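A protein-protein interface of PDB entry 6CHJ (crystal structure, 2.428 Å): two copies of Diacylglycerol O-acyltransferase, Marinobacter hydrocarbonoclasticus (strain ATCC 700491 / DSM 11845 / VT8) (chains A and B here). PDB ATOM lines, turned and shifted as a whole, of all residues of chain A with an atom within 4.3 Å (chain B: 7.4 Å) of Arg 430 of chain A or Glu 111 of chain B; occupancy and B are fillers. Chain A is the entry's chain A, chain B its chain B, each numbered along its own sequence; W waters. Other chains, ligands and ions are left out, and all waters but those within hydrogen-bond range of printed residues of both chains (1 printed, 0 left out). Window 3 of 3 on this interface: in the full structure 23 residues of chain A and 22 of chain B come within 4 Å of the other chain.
Water W1 lies within hydrogen-bond range of NH2 of Arg 112 of chain B (2.5 Å), OD2 of Asp 77 of chain B (2.5 Å) and O of Arg 429 of chain A (3.1 Å).
Of the printed residues of chain B, Arg 429 of chain A touches Asp 77 (3.8 Å). Arg 430 of chain A touches two residues of chain B. Ser 62 of chain B touches none of the printed residues of chain A. Of the printed residues of chain A, Asp 77 of chain B touches Arg 429 (3.8 Å). Of the printed residues of chain A, Glu 111 of chain B touches Ile 235 (3.9 Å), Thr 236 (3.8 Å) and Arg 430 (3.2 Å). The nearest residue of chain B that does not touch Arg 430 of chain A is Arg 60 of chain B (5.1 Å). The nearest printed residue of chain A that does not touch Glu 111 of chain B is Lys 234 of chain A (5.4 Å). The nearest printed residue of chain A that does not touch Arg 112 of chain B is Arg 429 of chain A (4.1 Å).
Among the printed residues, pairs that only touch across the chains: Thr 236 of chain A with Asp 109 of chain B, Arg 430 of chain A with Arg 112 of chain B, Thr 236 of chain A with Glu 111 of chain B and Ile 235 of chain A with Glu 111 of chain B.
The backbone carbonyl oxygen (O) of Lys 234 of chain A is in hydrogen-bond range of the guanidinium group (NH2) of Arg 430 of chain A, at 3.1 Å. The side-chain sulfur (SG) of Cys 428 of chain A is in hydrogen-bond range of the side-chain hydroxyl (OG1) of Thr 236 of chain A (3.3 Å). SG of Cys 428 of chain A sits close to N of Arg 430 of chain A, at 3.5 Å. NH1 of Arg 60 of chain B lies within salt-bridge range of OE2 of Glu 111 of chain B, at 3.6 Å. The backbone NH (N) of His 80 of chain B sits at hydrogen-bond distance from the side-chain carboxylate (OD1) of Asp 77 of chain B, at 3.3 Å. A ring nitrogen (ND1) of His 81 of chain B lies within hydrogen-bond range of the backbone carbonyl oxygen (O) of Asp 77 of chain B (3.3 Å).
The side-chain carboxylate of Asp 77 of chain B is in salt-bridge range of the guanidinium group of Arg 429 of chain A (3.8 Å). OE1 of Glu 111 of chain B is in salt-bridge range of NH1 of Arg 430 of chain A (3.2 Å).
Along chain A the printed residues that touch a printed residue of chain B span positions 235 to 430. Among the printed residues, 6 pairs touch across the chains. Among the printed residues, Asp or Glu carboxylates within 4 Å of a Lys or Arg side-chain nitrogen of the other chain: Arg 429 of chain A with Asp 77 of chain B (3.8 Å) and Arg 430 of chain A with Glu 111 of chain B (3.2 Å).
No position is printed for both chains. Of the 6 pairs that touch across the chains among the printed residues, none has its exchanged pair printed and touching as well.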
ATOM      1  N   LYS A 234      -6.262  16.835 -18.525  1.00  0.00           N
ATOM      2  CA  LYS A 234      -7.166  17.953 -18.721  1.00  0.00           C
ATOM      3  C   LYS A 234      -6.414  19.275 -18.545  1.00  0.00           C
ATOM      4  O   LYS A 234      -5.522  19.394 -17.705  1.00  0.00           O
ATOM      5  CB  LYS A 234      -8.323  17.865 -17.723  1.00  0.00           C
ATOM      6  CG  LYS A 234      -9.341  16.741 -18.043  1.00  0.00           C
ATOM      7  CD  LYS A 234     -10.773  17.073 -17.614  1.00  0.00           C
ATOM      8  CE  LYS A 234     -11.722  17.365 -18.826  1.00  0.00           C
ATOM      9  NZ  LYS A 234     -12.303  16.119 -19.515  1.00  0.00           N
ATOM     10  N   ILE A 235      -6.778  20.276 -19.346  1.00  0.00           N
ATOM     11  CA  ILE A 235      -6.042  21.538 -19.405  1.00  0.00           C
ATOM     12  C   ILE A 235      -6.933  22.688 -18.954  1.00  0.00           C
ATOM     13  O   ILE A 235      -8.129  22.535 -18.699  1.00  0.00           O
ATOM     14  CB  ILE A 235      -5.485  21.847 -20.816  1.00  0.00           C
ATOM     15  CG1 ILE A 235      -6.627  22.152 -21.788  1.00  0.00           C
ATOM     16  CG2 ILE A 235      -4.571  20.714 -21.320  1.00  0.00           C
ATOM     17  CD1 ILE A 235      -6.158  22.374 -23.211  1.00  0.00           C
ATOM     18  N   THR A 236      -6.309  23.846 -18.830  1.00  0.00           N
ATOM     19  CA  THR A 236      -6.965  25.131 -18.661  1.00  0.00           C
ATOM     20  C   THR A 236      -6.955  25.868 -19.990  1.00  0.00           C
ATOM     21  O   THR A 236      -6.254  25.486 -20.933  1.00  0.00           O
ATOM     22  CB  THR A 236      -6.235  25.938 -17.598  1.00  0.00           C
ATOM     23  OG1 THR A 236      -5.013  26.443 -18.156  1.00  0.00           O
ATOM     24  CG2 THR A 236      -5.883  25.030 -16.434  1.00  0.00           C
ATOM     25  N   CYS A 428      -0.738  24.499 -22.670  1.00  0.00           N
ATOM     26  CA  CYS A 428      -1.495  24.983 -21.524  1.00  0.00           C
ATOM     27  C   CYS A 428      -0.524  25.476 -20.458  1.00  0.00           C
ATOM     28  O   CYS A 428       0.428  24.771 -20.090  1.00  0.00           O
ATOM     29  CB  CYS A 428      -2.410  23.896 -20.963  1.00  0.00           C
ATOM     30  SG  CYS A 428      -2.894  24.099 -19.204  1.00  0.00           S
ATOM     31  N   ARG A 429      -0.766  26.703 -19.972  1.00  0.00           N
ATOM     32  CA  ARG A 429       0.200  27.369 -19.099  1.00  0.00           C
ATOM     33  C   ARG A 429       0.342  26.660 -17.754  1.00  0.00           C
ATOM     34  O   ARG A 429       1.429  26.638 -17.174  1.00  0.00           O
ATOM     35  CB  ARG A 429      -0.209  28.836 -18.911  1.00  0.00           C
ATOM     36  CG  ARG A 429       0.627  29.605 -17.918  1.00  0.00           C
ATOM     37  CD  ARG A 429       0.356  31.117 -17.950  1.00  0.00           C
ATOM     38  NE  ARG A 429       1.617  31.854 -17.819  1.00  0.00           N
ATOM     39  CZ  ARG A 429       2.243  32.501 -18.806  1.00  0.00           C
ATOM     40  NH1 ARG A 429       1.729  32.585 -20.032  1.00  0.00           N
ATOM     41  NH2 ARG A 429       3.389  33.097 -18.552  1.00  0.00           N
ATOM     42  N   ARG A 430      -0.740  26.075 -17.244  1.00  0.00           N
ATOM     43  CA  ARG A 430      -0.669  25.390 -15.961  1.00  0.00           C
ATOM     44  C   ARG A 430      -0.052  23.995 -16.100  1.00  0.00           C
ATOM     45  O   ARG A 430       0.725  23.568 -15.238  1.00  0.00           O
ATOM     46  CB  ARG A 430      -2.069  25.306 -15.339  1.00  0.00           C
ATOM     47  CG  ARG A 430      -2.095  24.741 -13.913  1.00  0.00           C
ATOM     48  CD  ARG A 430      -3.453  24.162 -13.550  1.00  0.00           C
ATOM     49  NE  ARG A 430      -3.812  23.093 -14.474  1.00  0.00           N
ATOM     50  CZ  ARG A 430      -4.988  22.468 -14.512  1.00  0.00           C
ATOM     51  NH1 ARG A 430      -5.962  22.793 -13.669  1.00  0.00           N
ATOM     52  NH2 ARG A 430      -5.194  21.517 -15.419  1.00  0.00           N
ATOM     53  N   THR A 431      -0.375  23.280 -17.182  1.00  0.00           N
ATOM     54  CA  THR A 431       0.130  21.927 -17.357  1.00  0.00           C
ATOM     55  C   THR A 431       1.602  21.928 -17.709  1.00  0.00           C
ATOM     56  O   THR A 431       2.332  20.990 -17.365  1.00  0.00           O
ATOM     57  CB  THR A 431      -0.647  21.200 -18.450  1.00  0.00           C
ATOM     58  OG1 THR A 431      -2.045  21.207 -18.126  1.00  0.00           O
ATOM     59  CG2 THR A 431      -0.156  19.749 -18.564  1.00  0.00           C
ATOM     60  N   LEU A 432       2.051  22.967 -18.401  1.00  0.00           N
ATOM     61  CA  LEU A 432       3.415  23.063 -18.893  1.00  0.00           C
ATOM     62  C   LEU A 432       4.023  24.309 -18.258  1.00  0.00           C
ATOM     63  O   LEU A 432       4.064  25.394 -18.869  1.00  0.00           O
ATOM     64  CB  LEU A 432       3.425  23.049 -20.420  1.00  0.00           C
ATOM     65  CG  LEU A 432       2.855  21.679 -20.863  1.00  0.00           C
ATOM     66  CD1 LEU A 432       2.182  21.714 -22.213  1.00  0.00           C
ATOM     67  CD2 LEU A 432       3.936  20.606 -20.839  1.00  0.00           C
ATOM     68  N   PRO A 433       4.451  24.200 -16.998  1.00  0.00           N
ATOM     69  CA  PRO A 433       5.177  25.302 -16.357  1.00  0.00           C
ATOM     70  C   PRO A 433       6.530  25.505 -17.023  1.00  0.00           C
ATOM     71  O   PRO A 433       7.263  24.543 -17.269  1.00  0.00           O
ATOM     72  CB  PRO A 433       5.328  24.828 -14.907  1.00  0.00           C
ATOM     73  CG  PRO A 433       5.259  23.333 -14.993  1.00  0.00           C
ATOM     74  CD  PRO A 433       4.252  23.066 -16.073  1.00  0.00           C
ATOM     75  N   GLN B  59      -8.158  31.584  -3.483  1.00  0.00           N
ATOM     76  CA  GLN B  59      -9.255  30.639  -3.577  1.00  0.00           C
ATOM     77  C   GLN B  59      -9.466  30.252  -5.033  1.00  0.00           C
ATOM     78  O   GLN B  59      -9.322  31.077  -5.932  1.00  0.00           O
ATOM     79  CB  GLN B  59     -10.529  31.270  -3.004  1.00  0.00           C
ATOM     80  CG  GLN B  59     -10.392  31.705  -1.553  1.00  0.00           C
ATOM     81  CD  GLN B  59     -10.145  30.517  -0.632  1.00  0.00           C
ATOM     82  OE1 GLN B  59     -10.866  29.514  -0.688  1.00  0.00           O
ATOM     83  NE2 GLN B  59      -9.113  30.616   0.206  1.00  0.00           N
ATOM     84  N   ARG B  60      -9.821  29.001  -5.272  1.00  0.00           N
ATOM     85  CA  ARG B  60     -10.113  28.609  -6.636  1.00  0.00           C
ATOM     86  C   ARG B  60     -11.303  27.673  -6.629  1.00  0.00           C
ATOM     87  O   ARG B  60     -11.592  27.021  -5.624  1.00  0.00           O
ATOM     88  CB  ARG B  60      -8.893  27.975  -7.321  1.00  0.00           C
ATOM     89  CG  ARG B  60      -8.750  26.497  -7.158  1.00  0.00           C
ATOM     90  CD  ARG B  60      -7.624  25.985  -8.044  1.00  0.00           C
ATOM     91  NE  ARG B  60      -7.754  24.556  -8.322  1.00  0.00           N
ATOM     92  CZ  ARG B  60      -8.644  24.024  -9.161  1.00  0.00           C
ATOM     93  NH1 ARG B  60      -9.506  24.800  -9.823  1.00  0.00           N
ATOM     94  NH2 ARG B  60      -8.677  22.707  -9.331  1.00  0.00           N
ATOM     95  N   LEU B  61     -12.011  27.640  -7.752  1.00  0.00           N
ATOM     96  CA  LEU B  61     -13.242  26.875  -7.838  1.00  0.00           C
ATOM     97  C   LEU B  61     -12.941  25.393  -7.992  1.00  0.00           C
ATOM     98  O   LEU B  61     -12.069  24.994  -8.769  1.00  0.00           O
ATOM     99  CB  LEU B  61     -14.110  27.365  -9.000  1.00  0.00           C
ATOM    100  CG  LEU B  61     -15.516  26.751  -9.083  1.00  0.00           C
ATOM    101  CD1 LEU B  61     -16.327  27.009  -7.810  1.00  0.00           C
ATOM    102  CD2 LEU B  61     -16.280  27.217 -10.329  1.00  0.00           C
ATOM    103  N   SER B  62     -13.663  24.579  -7.225  1.00  0.00           N
ATOM    104  CA  SER B  62     -13.588  23.133  -7.334  1.00  0.00           C
ATOM    105  C   SER B  62     -14.954  22.577  -6.973  1.00  0.00           C
ATOM    106  O   SER B  62     -15.758  23.243  -6.318  1.00  0.00           O
ATOM    107  CB  SER B  62     -12.505  22.556  -6.424  1.00  0.00           C
ATOM    108  OG  SER B  62     -11.969  21.371  -6.977  1.00  0.00           O
ATOM    109  N   ASP B  73      -5.617  27.441  -3.334  1.00  0.00           N
ATOM    110  CA  ASP B  73      -4.849  27.103  -4.525  1.00  0.00           C
ATOM    111  C   ASP B  73      -3.396  26.855  -4.145  1.00  0.00           C
ATOM    112  O   ASP B  73      -2.680  27.780  -3.750  1.00  0.00           O
ATOM    113  CB  ASP B  73      -4.960  28.202  -5.574  1.00  0.00           C
ATOM    114  CG  ASP B  73      -4.507  27.732  -6.945  1.00  0.00           C
ATOM    115  OD1 ASP B  73      -4.716  26.541  -7.252  1.00  0.00           O
ATOM    116  OD2 ASP B  73      -3.943  28.541  -7.711  1.00  0.00           O
ATOM    117  N   HIS B  75      -0.807  25.856  -6.106  1.00  0.00           N
ATOM    118  CA  HIS B  75       0.167  26.306  -7.102  1.00  0.00           C
ATOM    119  C   HIS B  75      -0.420  27.476  -7.892  1.00  0.00           C
ATOM    120  O   HIS B  75      -0.955  27.292  -8.992  1.00  0.00           O
ATOM    121  CB  HIS B  75       0.595  25.124  -8.051  1.00  0.00           C
ATOM    122  CG  HIS B  75       0.563  23.771  -7.404  1.00  0.00           C
ATOM    123  ND1 HIS B  75      -0.611  23.080  -7.181  1.00  0.00           N
ATOM    124  CD2 HIS B  75       1.559  22.979  -6.942  1.00  0.00           C
ATOM    125  CE1 HIS B  75      -0.337  21.925  -6.602  1.00  0.00           C
ATOM    126  NE2 HIS B  75       0.971  21.839  -6.445  1.00  0.00           N
ATOM    127  N   ASP B  77       0.243  30.861 -10.055  1.00  0.00           N
ATOM    128  CA  ASP B  77       1.268  31.366 -10.963  1.00  0.00           C
ATOM    129  C   ASP B  77       1.071  32.879 -11.091  1.00  0.00           C
ATOM    130  O   ASP B  77       0.225  33.345 -11.870  1.00  0.00           O
ATOM    131  CB  ASP B  77       1.148  30.624 -12.291  1.00  0.00           C
ATOM    132  CG  ASP B  77       2.076  31.152 -13.376  1.00  0.00           C
ATOM    133  OD1 ASP B  77       2.621  32.266 -13.261  1.00  0.00           O
ATOM    134  OD2 ASP B  77       2.232  30.430 -14.387  1.00  0.00           O
ATOM    135  N   HIS B  80       0.588  34.606 -14.278  1.00  0.00           N
ATOM    136  CA  HIS B  80      -0.716  34.529 -14.923  1.00  0.00           C
ATOM    137  C   HIS B  80      -1.645  35.645 -14.447  1.00  0.00           C
ATOM    138  O   HIS B  80      -2.337  36.262 -15.263  1.00  0.00           O
ATOM    139  CB  HIS B  80      -1.376  33.171 -14.672  1.00  0.00           C
ATOM    140  CG  HIS B  80      -2.773  33.099 -15.185  1.00  0.00           C
ATOM    141  ND1 HIS B  80      -3.062  32.900 -16.522  1.00  0.00           N
ATOM    142  CD2 HIS B  80      -3.961  33.250 -14.553  1.00  0.00           C
ATOM    143  CE1 HIS B  80      -4.375  32.921 -16.682  1.00  0.00           C
ATOM    144  NE2 HIS B  80      -4.941  33.136 -15.507  1.00  0.00           N
ATOM    145  N   HIS B  81      -1.680  35.921 -13.135  1.00  0.00           N
ATOM    146  CA  HIS B  81      -2.639  36.884 -12.599  1.00  0.00           C
ATOM    147  C   HIS B  81      -2.154  38.335 -12.713  1.00  0.00           C
ATOM    148  O   HIS B  81      -2.972  39.247 -12.873  1.00  0.00           O
ATOM    149  CB  HIS B  81      -2.960  36.544 -11.138  1.00  0.00           C
ATOM    150  CG  HIS B  81      -3.562  35.186 -10.941  1.00  0.00           C
ATOM    151  ND1 HIS B  81      -2.803  34.037 -10.856  1.00  0.00           N
ATOM    152  CD2 HIS B  81      -4.849  34.796 -10.782  1.00  0.00           C
ATOM    153  CE1 HIS B  81      -3.599  32.997 -10.665  1.00  0.00           C
ATOM    154  NE2 HIS B  81      -4.845  33.430 -10.615  1.00  0.00           N
ATOM    155  N   MET B 108     -12.777  34.985 -17.824  1.00  0.00           N
ATOM    156  CA  MET B 108     -11.684  34.543 -16.977  1.00  0.00           C
ATOM    157  C   MET B 108     -11.652  33.022 -16.923  1.00  0.00           C
ATOM    158  O   MET B 108     -12.661  32.351 -17.115  1.00  0.00           O
ATOM    159  CB  MET B 108     -11.810  35.103 -15.563  1.00  0.00           C
ATOM    160  CG  MET B 108     -12.256  36.515 -15.501  1.00  0.00           C
ATOM    161  SD  MET B 108     -12.143  37.222 -13.856  1.00  0.00           S
ATOM    162  CE  MET B 108     -10.345  37.177 -13.671  1.00  0.00           C
ATOM    163  N   ASP B 109     -10.473  32.488 -16.626  1.00  0.00           N
ATOM    164  CA  ASP B 109     -10.259  31.047 -16.531  1.00  0.00           C
ATOM    165  C   ASP B 109     -10.764  30.532 -15.185  1.00  0.00           C
ATOM    166  O   ASP B 109     -10.282  30.965 -14.133  1.00  0.00           O
ATOM    167  CB  ASP B 109      -8.769  30.770 -16.692  1.00  0.00           C
ATOM    168  CG  ASP B 109      -8.436  29.299 -16.735  1.00  0.00           C
ATOM    169  OD1 ASP B 109      -9.331  28.428 -16.905  1.00  0.00           O
ATOM    170  OD2 ASP B 109      -7.230  29.032 -16.616  1.00  0.00           O
ATOM    171  N   ARG B 110     -11.710  29.595 -15.207  1.00  0.00           N
ATOM    172  CA  ARG B 110     -12.293  29.129 -13.948  1.00  0.00           C
ATOM    173  C   ARG B 110     -11.379  28.194 -13.165  1.00  0.00           C
ATOM    174  O   ARG B 110     -11.624  27.966 -11.974  1.00  0.00           O
ATOM    175  CB  ARG B 110     -13.627  28.436 -14.207  1.00  0.00           C
ATOM    176  CG  ARG B 110     -14.805  29.382 -14.090  1.00  0.00           C
ATOM    177  CD  ARG B 110     -16.124  28.676 -14.280  1.00  0.00           C
ATOM    178  NE  ARG B 110     -17.140  29.664 -14.589  1.00  0.00           N
ATOM    179  CZ  ARG B 110     -18.422  29.408 -14.797  1.00  0.00           C
ATOM    180  NH1 ARG B 110     -18.880  28.159 -14.739  1.00  0.00           N
ATOM    181  NH2 ARG B 110     -19.246  30.423 -15.051  1.00  0.00           N
ATOM    182  N   GLU B 111     -10.336  27.654 -13.793  1.00  0.00           N
ATOM    183  CA  GLU B 111      -9.454  26.706 -13.133  1.00  0.00           C
ATOM    184  C   GLU B 111      -8.404  27.376 -12.242  1.00  0.00           C
ATOM    185  O   GLU B 111      -7.669  26.668 -11.537  1.00  0.00           O
ATOM    186  CB  GLU B 111      -8.789  25.814 -14.185  1.00  0.00           C
ATOM    187  CG  GLU B 111      -9.724  24.735 -14.775  1.00  0.00           C
ATOM    188  CD  GLU B 111      -9.499  23.349 -14.158  1.00  0.00           C
ATOM    189  OE1 GLU B 111      -8.946  22.454 -14.840  1.00  0.00           O
ATOM    190  OE2 GLU B 111      -9.868  23.157 -12.980  1.00  0.00           O
ATOM    191  N   ARG B 112      -8.316  28.701 -12.237  1.00  0.00           N
ATOM    192  CA  ARG B 112      -7.436  29.432 -11.341  1.00  0.00           C
ATOM    193  C   ARG B 112      -8.235  30.471 -10.581  1.00  0.00           C
ATOM    194  O   ARG B 112      -9.340  30.836 -10.997  1.00  0.00           O
ATOM    195  CB  ARG B 112      -6.300  30.103 -12.116  1.00  0.00           C
ATOM    196  CG  ARG B 112      -5.758  29.221 -13.200  1.00  0.00           C
ATOM    197  CD  ARG B 112      -4.617  29.904 -13.862  1.00  0.00           C
ATOM    198  NE  ARG B 112      -3.367  29.478 -13.249  1.00  0.00           N
ATOM    199  CZ  ARG B 112      -2.341  28.996 -13.932  1.00  0.00           C
ATOM    200  NH1 ARG B 112      -2.410  28.888 -15.253  1.00  0.00           N
ATOM    201  NH2 ARG B 112      -1.249  28.627 -13.290  1.00  0.00           N
ATOM    202  N   PRO B 113      -7.731  30.936  -9.437  1.00  0.00           N
ATOM    203  CA  PRO B 113      -8.394  32.047  -8.742  1.00  0.00           C
ATOM    204  C   PRO B 113      -8.692  33.164  -9.728  1.00  0.00           C
ATOM    205  O   PRO B 113      -7.874  33.492 -10.589  1.00  0.00           O
ATOM    206  CB  PRO B 113      -7.369  32.473  -7.680  1.00  0.00           C
ATOM    207  CG  PRO B 113      -6.099  31.736  -8.034  1.00  0.00           C
ATOM    208  CD  PRO B 113      -6.511  30.505  -8.739  1.00  0.00           C
ATOM    209  N   MET B 114      -9.897  33.704  -9.649  1.00  0.00           N
ATOM    210  CA  MET B 114     -10.425  34.480 -10.761  1.00  0.00           C
ATOM    211  C   MET B 114     -10.197  35.975 -10.535  1.00  0.00           C
ATOM    212  O   MET B 114     -11.121  36.772 -10.359  1.00  0.00           O
ATOM    213  CB  MET B 114     -11.887  34.133 -10.976  1.00  0.00           C
ATOM    214  CG  MET B 114     -12.089  32.635 -11.188  1.00  0.00           C
ATOM    215  SD  MET B 114     -13.741  32.190 -11.745  1.00  0.00           S
ATOM    216  CE  MET B 114     -14.424  31.419 -10.262  1.00  0.00           C
HETATM  217  O   HOH W   1       0.795  28.372 -14.744  1.00  0.00           O
